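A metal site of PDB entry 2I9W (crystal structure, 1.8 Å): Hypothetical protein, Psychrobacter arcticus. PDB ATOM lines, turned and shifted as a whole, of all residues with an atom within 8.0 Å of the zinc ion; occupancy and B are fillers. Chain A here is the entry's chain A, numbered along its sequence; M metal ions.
The zinc ion is bound by SG of Cys 168 (2.3 Å), SG of Cys 170 (2.4 Å), SG of Cys 180 (2.4 Å) and SG of Cys 179 (2.4 Å).
The zinc ion has four donor atoms within binding distance.
The side-chain hydroxyl (OG) of Ser 172 sits close to the side-chain sulfur (SG) of Cys 179.
The backbone NH (N) of Ser 172 lies close to the side-chain sulfur (SG) of Cys 170 (3.4 Å).
The backbone carbonyl oxygen of Glu 174 lies within hydrogen-bond range of the backbone NH of Cys 168, at 2.8 Å.
A ring nitrogen (NE2) of His 114 lies close to the side-chain sulfur (SG) of Cys 180.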
ATOM      1  N   LEU A  77      15.772  15.760  -4.137  1.00  0.00           N
ATOM      2  CA  LEU A  77      16.117  14.406  -3.691  1.00  0.00           C
ATOM      3  C   LEU A  77      15.454  14.131  -2.354  1.00  0.00           C
ATOM      4  O   LEU A  77      15.639  14.913  -1.426  1.00  0.00           O
ATOM      5  CB  LEU A  77      17.645  14.246  -3.534  1.00  0.00           C
ATOM      6  CG  LEU A  77      18.045  12.782  -3.271  1.00  0.00           C
ATOM      7  CD1 LEU A  77      17.914  11.970  -4.566  1.00  0.00           C
ATOM      8  CD2 LEU A  77      19.458  12.694  -2.738  1.00  0.00           C
ATOM      9  N   ARG A 113      22.262   7.156 -14.400  1.00  0.00           N
ATOM     10  CA  ARG A 113      21.103   7.654 -13.648  1.00  0.00           C
ATOM     11  C   ARG A 113      21.088   9.159 -13.397  1.00  0.00           C
ATOM     12  O   ARG A 113      20.196   9.672 -12.677  1.00  0.00           O
ATOM     13  CB  ARG A 113      20.962   6.885 -12.344  1.00  0.00           C
ATOM     14  CG  ARG A 113      22.145   6.995 -11.427  1.00  0.00           C
ATOM     15  CD  ARG A 113      22.125   5.897 -10.311  1.00  0.00           C
ATOM     16  NE  ARG A 113      21.684   4.535 -10.677  1.00  0.00           N
ATOM     17  CZ  ARG A 113      22.455   3.479 -11.001  1.00  0.00           C
ATOM     18  NH1 ARG A 113      23.785   3.526 -11.109  1.00  0.00           N
ATOM     19  NH2 ARG A 113      21.854   2.330 -11.269  1.00  0.00           N
ATOM     20  N   HIS A 114      22.050   9.895 -13.964  1.00  0.00           N
ATOM     21  CA  HIS A 114      22.108  11.346 -13.774  1.00  0.00           C
ATOM     22  C   HIS A 114      22.071  12.158 -15.054  1.00  0.00           C
ATOM     23  O   HIS A 114      22.445  11.689 -16.138  1.00  0.00           O
ATOM     24  CB  HIS A 114      23.382  11.763 -13.084  1.00  0.00           C
ATOM     25  CG  HIS A 114      23.537  11.174 -11.743  1.00  0.00           C
ATOM     26  ND1 HIS A 114      24.179   9.978 -11.534  1.00  0.00           N
ATOM     27  CD2 HIS A 114      23.149  11.618 -10.526  1.00  0.00           C
ATOM     28  CE1 HIS A 114      24.157   9.691 -10.252  1.00  0.00           C
ATOM     29  NE2 HIS A 114      23.572  10.680  -9.610  1.00  0.00           N
ATOM     30  N   VAL A 139      19.006  13.400 -10.472  1.00  0.00           N
ATOM     31  CA  VAL A 139      19.071  11.934 -10.402  1.00  0.00           C
ATOM     32  C   VAL A 139      17.687  11.384 -10.679  1.00  0.00           C
ATOM     33  O   VAL A 139      16.687  11.942 -10.224  1.00  0.00           O
ATOM     34  CB  VAL A 139      19.643  11.405  -9.059  1.00  0.00           C
ATOM     35  CG1 VAL A 139      18.726  11.726  -7.873  1.00  0.00           C
ATOM     36  CG2 VAL A 139      19.951   9.900  -9.159  1.00  0.00           C
ATOM     37  N   LYS A 140      17.658  10.284 -11.424  1.00  0.00           N
ATOM     38  CA  LYS A 140      16.466   9.514 -11.718  1.00  0.00           C
ATOM     39  C   LYS A 140      16.329   8.395 -10.683  1.00  0.00           C
ATOM     40  O   LYS A 140      17.252   7.554 -10.528  1.00  0.00           O
ATOM     41  CB  LYS A 140      16.522   8.948 -13.147  1.00  0.00           C
ATOM     42  CG  LYS A 140      15.171   8.894 -13.855  1.00  0.00           C
ATOM     43  CD  LYS A 140      15.241   8.344 -15.291  1.00  0.00           C
ATOM     44  CE  LYS A 140      14.055   8.866 -16.143  1.00  0.00           C
ATOM     45  N   ILE A 141      15.178   8.376 -10.019  1.00  0.00           N
ATOM     46  CA  ILE A 141      14.801   7.406  -9.004  1.00  0.00           C
ATOM     47  C   ILE A 141      13.481   6.710  -9.344  1.00  0.00           C
ATOM     48  O   ILE A 141      12.496   7.371  -9.647  1.00  0.00           O
ATOM     49  CB  ILE A 141      14.640   8.047  -7.629  1.00  0.00           C
ATOM     50  CG1 ILE A 141      15.942   8.745  -7.173  1.00  0.00           C
ATOM     51  CG2 ILE A 141      14.193   6.972  -6.619  1.00  0.00           C
ATOM     52  CD1 ILE A 141      15.678   9.658  -5.919  1.00  0.00           C
ATOM     53  N   LEU A 154      19.487  17.354  -7.190  1.00  0.00           N
ATOM     54  CA  LEU A 154      20.542  17.135  -6.159  1.00  0.00           C
ATOM     55  C   LEU A 154      20.958  18.511  -5.639  1.00  0.00           C
ATOM     56  O   LEU A 154      21.588  19.293  -6.356  1.00  0.00           O
ATOM     57  CB  LEU A 154      21.749  16.404  -6.766  1.00  0.00           C
ATOM     58  CG  LEU A 154      21.573  14.945  -7.153  1.00  0.00           C
ATOM     59  CD1 LEU A 154      22.923  14.393  -7.644  1.00  0.00           C
ATOM     60  CD2 LEU A 154      20.998  14.084  -6.050  1.00  0.00           C
ATOM     61  N   PRO A 167      25.802   3.035   0.893  1.00  0.00           N
ATOM     62  CA  PRO A 167      24.910   3.208  -0.234  1.00  0.00           C
ATOM     63  C   PRO A 167      24.421   4.645  -0.436  1.00  0.00           C
ATOM     64  O   PRO A 167      24.161   5.382   0.523  1.00  0.00           O
ATOM     65  CB  PRO A 167      23.725   2.275   0.117  1.00  0.00           C
ATOM     66  CG  PRO A 167      24.294   1.261   1.001  1.00  0.00           C
ATOM     67  CD  PRO A 167      25.297   2.018   1.820  1.00  0.00           C
ATOM     68  N   CYS A 168      24.247   5.004  -1.693  1.00  0.00           N
ATOM     69  CA  CYS A 168      23.938   6.368  -2.031  1.00  0.00           C
ATOM     70  C   CYS A 168      22.585   6.774  -1.448  1.00  0.00           C
ATOM     71  O   CYS A 168      21.658   5.962  -1.354  1.00  0.00           O
ATOM     72  CB  CYS A 168      23.905   6.566  -3.543  1.00  0.00           C
ATOM     73  SG  CYS A 168      23.930   8.278  -3.945  1.00  0.00           S
ATOM     74  N   ILE A 169      22.514   8.039  -1.043  1.00  0.00           N
ATOM     75  CA  ILE A 169      21.312   8.657  -0.543  1.00  0.00           C
ATOM     76  C   ILE A 169      20.144   8.658  -1.527  1.00  0.00           C
ATOM     77  O   ILE A 169      19.026   8.833  -1.102  1.00  0.00           O
ATOM     78  CB  ILE A 169      21.553  10.109  -0.043  1.00  0.00           C
ATOM     79  CG1 ILE A 169      22.152  11.013  -1.145  1.00  0.00           C
ATOM     80  CG2 ILE A 169      22.473  10.044   1.176  1.00  0.00           C
ATOM     81  CD1 ILE A 169      22.343  12.500  -0.724  1.00  0.00           C
ATOM     82  N   CYS A 170      20.415   8.458  -2.815  1.00  0.00           N
ATOM     83  CA  CYS A 170      19.323   8.337  -3.815  1.00  0.00           C
ATOM     84  C   CYS A 170      18.663   6.989  -3.823  1.00  0.00           C
ATOM     85  O   CYS A 170      17.602   6.824  -4.406  1.00  0.00           O
ATOM     86  CB  CYS A 170      19.811   8.629  -5.231  1.00  0.00           C
ATOM     87  SG  CYS A 170      20.756   7.371  -6.007  1.00  0.00           S
ATOM     88  N   GLY A 171      19.305   5.997  -3.192  1.00  0.00           N
ATOM     89  CA  GLY A 171      18.717   4.648  -3.113  1.00  0.00           C
ATOM     90  C   GLY A 171      19.125   3.716  -4.244  1.00  0.00           C
ATOM     91  O   GLY A 171      18.606   2.611  -4.368  1.00  0.00           O
ATOM     92  N   SER A 172      20.095   4.131  -5.049  1.00  0.00           N
ATOM     93  CA  SER A 172      20.592   3.303  -6.170  1.00  0.00           C
ATOM     94  C   SER A 172      21.233   1.977  -5.782  1.00  0.00           C
ATOM     95  O   SER A 172      21.338   1.067  -6.635  1.00  0.00           O
ATOM     96  CB  SER A 172      21.654   4.098  -6.959  1.00  0.00           C
ATOM     97  OG  SER A 172      22.847   4.286  -6.187  1.00  0.00           O
ATOM     98  N   GLY A 173      21.748   1.900  -4.558  1.00  0.00           N
ATOM     99  CA  GLY A 173      22.587   0.766  -4.112  1.00  0.00           C
ATOM    100  C   GLY A 173      24.071   0.924  -4.394  1.00  0.00           C
ATOM    101  O   GLY A 173      24.881   0.191  -3.861  1.00  0.00           O
ATOM    102  N   GLU A 174      24.452   1.923  -5.200  1.00  0.00           N
ATOM    103  CA  GLU A 174      25.846   2.198  -5.538  1.00  0.00           C
ATOM    104  C   GLU A 174      26.415   2.969  -4.363  1.00  0.00           C
ATOM    105  O   GLU A 174      25.665   3.613  -3.628  1.00  0.00           O
ATOM    106  CB  GLU A 174      25.956   3.022  -6.822  1.00  0.00           C
ATOM    107  CG  GLU A 174      25.226   2.446  -8.030  1.00  0.00           C
ATOM    108  CD  GLU A 174      25.949   1.260  -8.629  1.00  0.00           C
ATOM    109  OE1 GLU A 174      25.771   0.120  -8.163  1.00  0.00           O
ATOM    110  OE2 GLU A 174      26.732   1.490  -9.578  1.00  0.00           O
ATOM    111  N   LYS A 175      27.724   2.893  -4.169  1.00  0.00           N
ATOM    112  CA  LYS A 175      28.360   3.696  -3.135  1.00  0.00           C
ATOM    113  C   LYS A 175      28.111   5.170  -3.423  1.00  0.00           C
ATOM    114  O   LYS A 175      28.235   5.601  -4.564  1.00  0.00           O
ATOM    115  CB  LYS A 175      29.871   3.446  -3.116  1.00  0.00           C
ATOM    116  CG  LYS A 175      30.284   2.003  -2.852  1.00  0.00           C
ATOM    117  CD  LYS A 175      31.778   1.820  -3.167  1.00  0.00           C
ATOM    118  CE  LYS A 175      32.226   0.368  -3.143  1.00  0.00           C
ATOM    119  NZ  LYS A 175      33.690   0.237  -3.401  1.00  0.00           N
ATOM    120  N   PHE A 176      27.828   5.955  -2.392  1.00  0.00           N
ATOM    121  CA  PHE A 176      27.670   7.402  -2.551  1.00  0.00           C
ATOM    122  C   PHE A 176      28.770   8.008  -3.442  1.00  0.00           C
ATOM    123  O   PHE A 176      28.490   8.750  -4.375  1.00  0.00           O
ATOM    124  CB  PHE A 176      27.628   8.069  -1.148  1.00  0.00           C
ATOM    125  CG  PHE A 176      27.444   9.559  -1.183  1.00  0.00           C
ATOM    126  CD1 PHE A 176      26.236  10.115  -1.629  1.00  0.00           C
ATOM    127  CD2 PHE A 176      28.476  10.410  -0.754  1.00  0.00           C
ATOM    128  CE1 PHE A 176      26.075  11.504  -1.668  1.00  0.00           C
ATOM    129  CE2 PHE A 176      28.317  11.793  -0.801  1.00  0.00           C
ATOM    130  CZ  PHE A 176      27.123  12.336  -1.224  1.00  0.00           C
ATOM    131  N   LYS A 177      30.024   7.685  -3.148  1.00  0.00           N
ATOM    132  CA  LYS A 177      31.172   8.181  -3.887  1.00  0.00           C
ATOM    133  C   LYS A 177      31.227   7.776  -5.383  1.00  0.00           C
ATOM    134  O   LYS A 177      31.927   8.422  -6.182  1.00  0.00           O
ATOM    135  CB  LYS A 177      32.470   7.786  -3.156  1.00  0.00           C
ATOM    136  CG  LYS A 177      32.780   6.324  -3.163  1.00  0.00           C
ATOM    137  CD  LYS A 177      34.043   5.999  -2.350  1.00  0.00           C
ATOM    138  CE  LYS A 177      35.324   6.480  -3.044  1.00  0.00           C
ATOM    139  NZ  LYS A 177      36.529   6.191  -2.192  1.00  0.00           N
ATOM    140  N   ARG A 178      30.489   6.740  -5.772  1.00  0.00           N
ATOM    141  CA  ARG A 178      30.406   6.275  -7.184  1.00  0.00           C
ATOM    142  C   ARG A 178      29.025   6.599  -7.765  1.00  0.00           C
ATOM    143  O   ARG A 178      28.592   6.015  -8.793  1.00  0.00           O
ATOM    144  CB  ARG A 178      30.658   4.768  -7.269  1.00  0.00           C
ATOM    145  CG  ARG A 178      32.133   4.373  -7.188  1.00  0.00           C
ATOM    146  CD  ARG A 178      32.912   4.578  -8.519  1.00  0.00           C
ATOM    147  NE  ARG A 178      32.548   3.628  -9.577  1.00  0.00           N
ATOM    148  CZ  ARG A 178      33.100   3.626 -10.805  1.00  0.00           C
ATOM    149  NH1 ARG A 178      34.038   4.522 -11.131  1.00  0.00           N
ATOM    150  NH2 ARG A 178      32.698   2.758 -11.719  1.00  0.00           N
ATOM    151  N   CYS A 179      28.324   7.512  -7.097  1.00  0.00           N
ATOM    152  CA  CYS A 179      26.940   7.842  -7.491  1.00  0.00           C
ATOM    153  C   CYS A 179      26.689   9.346  -7.331  1.00  0.00           C
ATOM    154  O   CYS A 179      27.354  10.097  -7.987  1.00  0.00           O
ATOM    155  CB  CYS A 179      25.887   7.002  -6.755  1.00  0.00           C
ATOM    156  SG  CYS A 179      24.221   6.961  -7.481  1.00  0.00           S
ATOM    157  N   CYS A 180      25.783   9.764  -6.457  1.00  0.00           N
ATOM    158  CA  CYS A 180      25.450  11.199  -6.365  1.00  0.00           C
ATOM    159  C   CYS A 180      26.606  12.037  -5.809  1.00  0.00           C
ATOM    160  O   CYS A 180      26.704  13.231  -6.096  1.00  0.00           O
ATOM    161  CB  CYS A 180      24.155  11.389  -5.585  1.00  0.00           C
ATOM    162  SG  CYS A 180      22.692  10.704  -6.440  1.00  0.00           S
ATOM    163  N   GLY A 181      27.495  11.394  -5.055  1.00  0.00           N
ATOM    164  CA  GLY A 181      28.714  12.034  -4.529  1.00  0.00           C
ATOM    165  C   GLY A 181      29.733  12.415  -5.591  1.00  0.00           C
ATOM    166  O   GLY A 181      30.631  13.223  -5.304  1.00  0.00           O
ATOM    167  N   MET A 182      29.645  11.844  -6.804  1.00  0.00           N
ATOM    168  CA  MET A 182      30.412  12.303  -7.951  1.00  0.00           C
ATOM    169  C   MET A 182      30.072  13.750  -8.299  1.00  0.00           C
ATOM    170  O   MET A 182      30.880  14.484  -8.869  1.00  0.00           O
ATOM    171  CB  MET A 182      30.134  11.456  -9.202  1.00  0.00           C
ATOM    172  CG  MET A 182      30.581  10.006  -9.216  1.00  0.00           C
ATOM    173  SD  MET A 182      32.511   9.819  -9.111  1.00  0.00           S
ATOM    174  CE  MET A 182      33.003  11.417 -10.123  1.00  0.00           C
ATOM    175  N   TYR A 183      28.851  14.169  -7.964  1.00  0.00           N
ATOM    176  CA  TYR A 183      28.309  15.416  -8.487  1.00  0.00           C
ATOM    177  C   TYR A 183      27.930  16.417  -7.407  1.00  0.00           C
ATOM    178  O   TYR A 183      27.928  17.617  -7.703  1.00  0.00           O
ATOM    179  CB  TYR A 183      27.134  15.133  -9.412  1.00  0.00           C
ATOM    180  CG  TYR A 183      27.439  14.088 -10.454  1.00  0.00           C
ATOM    181  CD1 TYR A 183      28.336  14.354 -11.477  1.00  0.00           C
ATOM    182  CD2 TYR A 183      26.838  12.823 -10.419  1.00  0.00           C
ATOM    183  CE1 TYR A 183      28.643  13.395 -12.453  1.00  0.00           C
ATOM    184  CE2 TYR A 183      27.144  11.850 -11.399  1.00  0.00           C
ATOM    185  CZ  TYR A 183      28.026  12.162 -12.430  1.00  0.00           C
ATOM    186  OH  TYR A 183      28.387  11.224 -13.410  1.00  0.00           O
ATOM    187  N   ILE A 184      27.611  15.966  -6.194  1.00  0.00           N
ATOM    188  CA  ILE A 184      27.447  16.858  -5.017  1.00  0.00           C
ATOM    189  C   ILE A 184      28.291  16.411  -3.832  1.00  0.00           C
ATOM    190  O   ILE A 184      28.327  17.077  -2.797  1.00  0.00           O
ATOM    191  CB  ILE A 184      25.987  16.975  -4.522  1.00  0.00           C
ATOM    192  CG1 ILE A 184      25.500  15.662  -3.907  1.00  0.00           C
ATOM    193  CG2 ILE A 184      25.090  17.460  -5.645  1.00  0.00           C
ATOM    194  CD1 ILE A 184      24.108  15.730  -3.368  1.00  0.00           C
ATOM    195  OXT ILE A 184      28.947  15.365  -3.884  1.00  0.00           O
HETATM  196 ZN    ZN M   1      22.899   8.378  -6.024  1.00  0.00          ZN
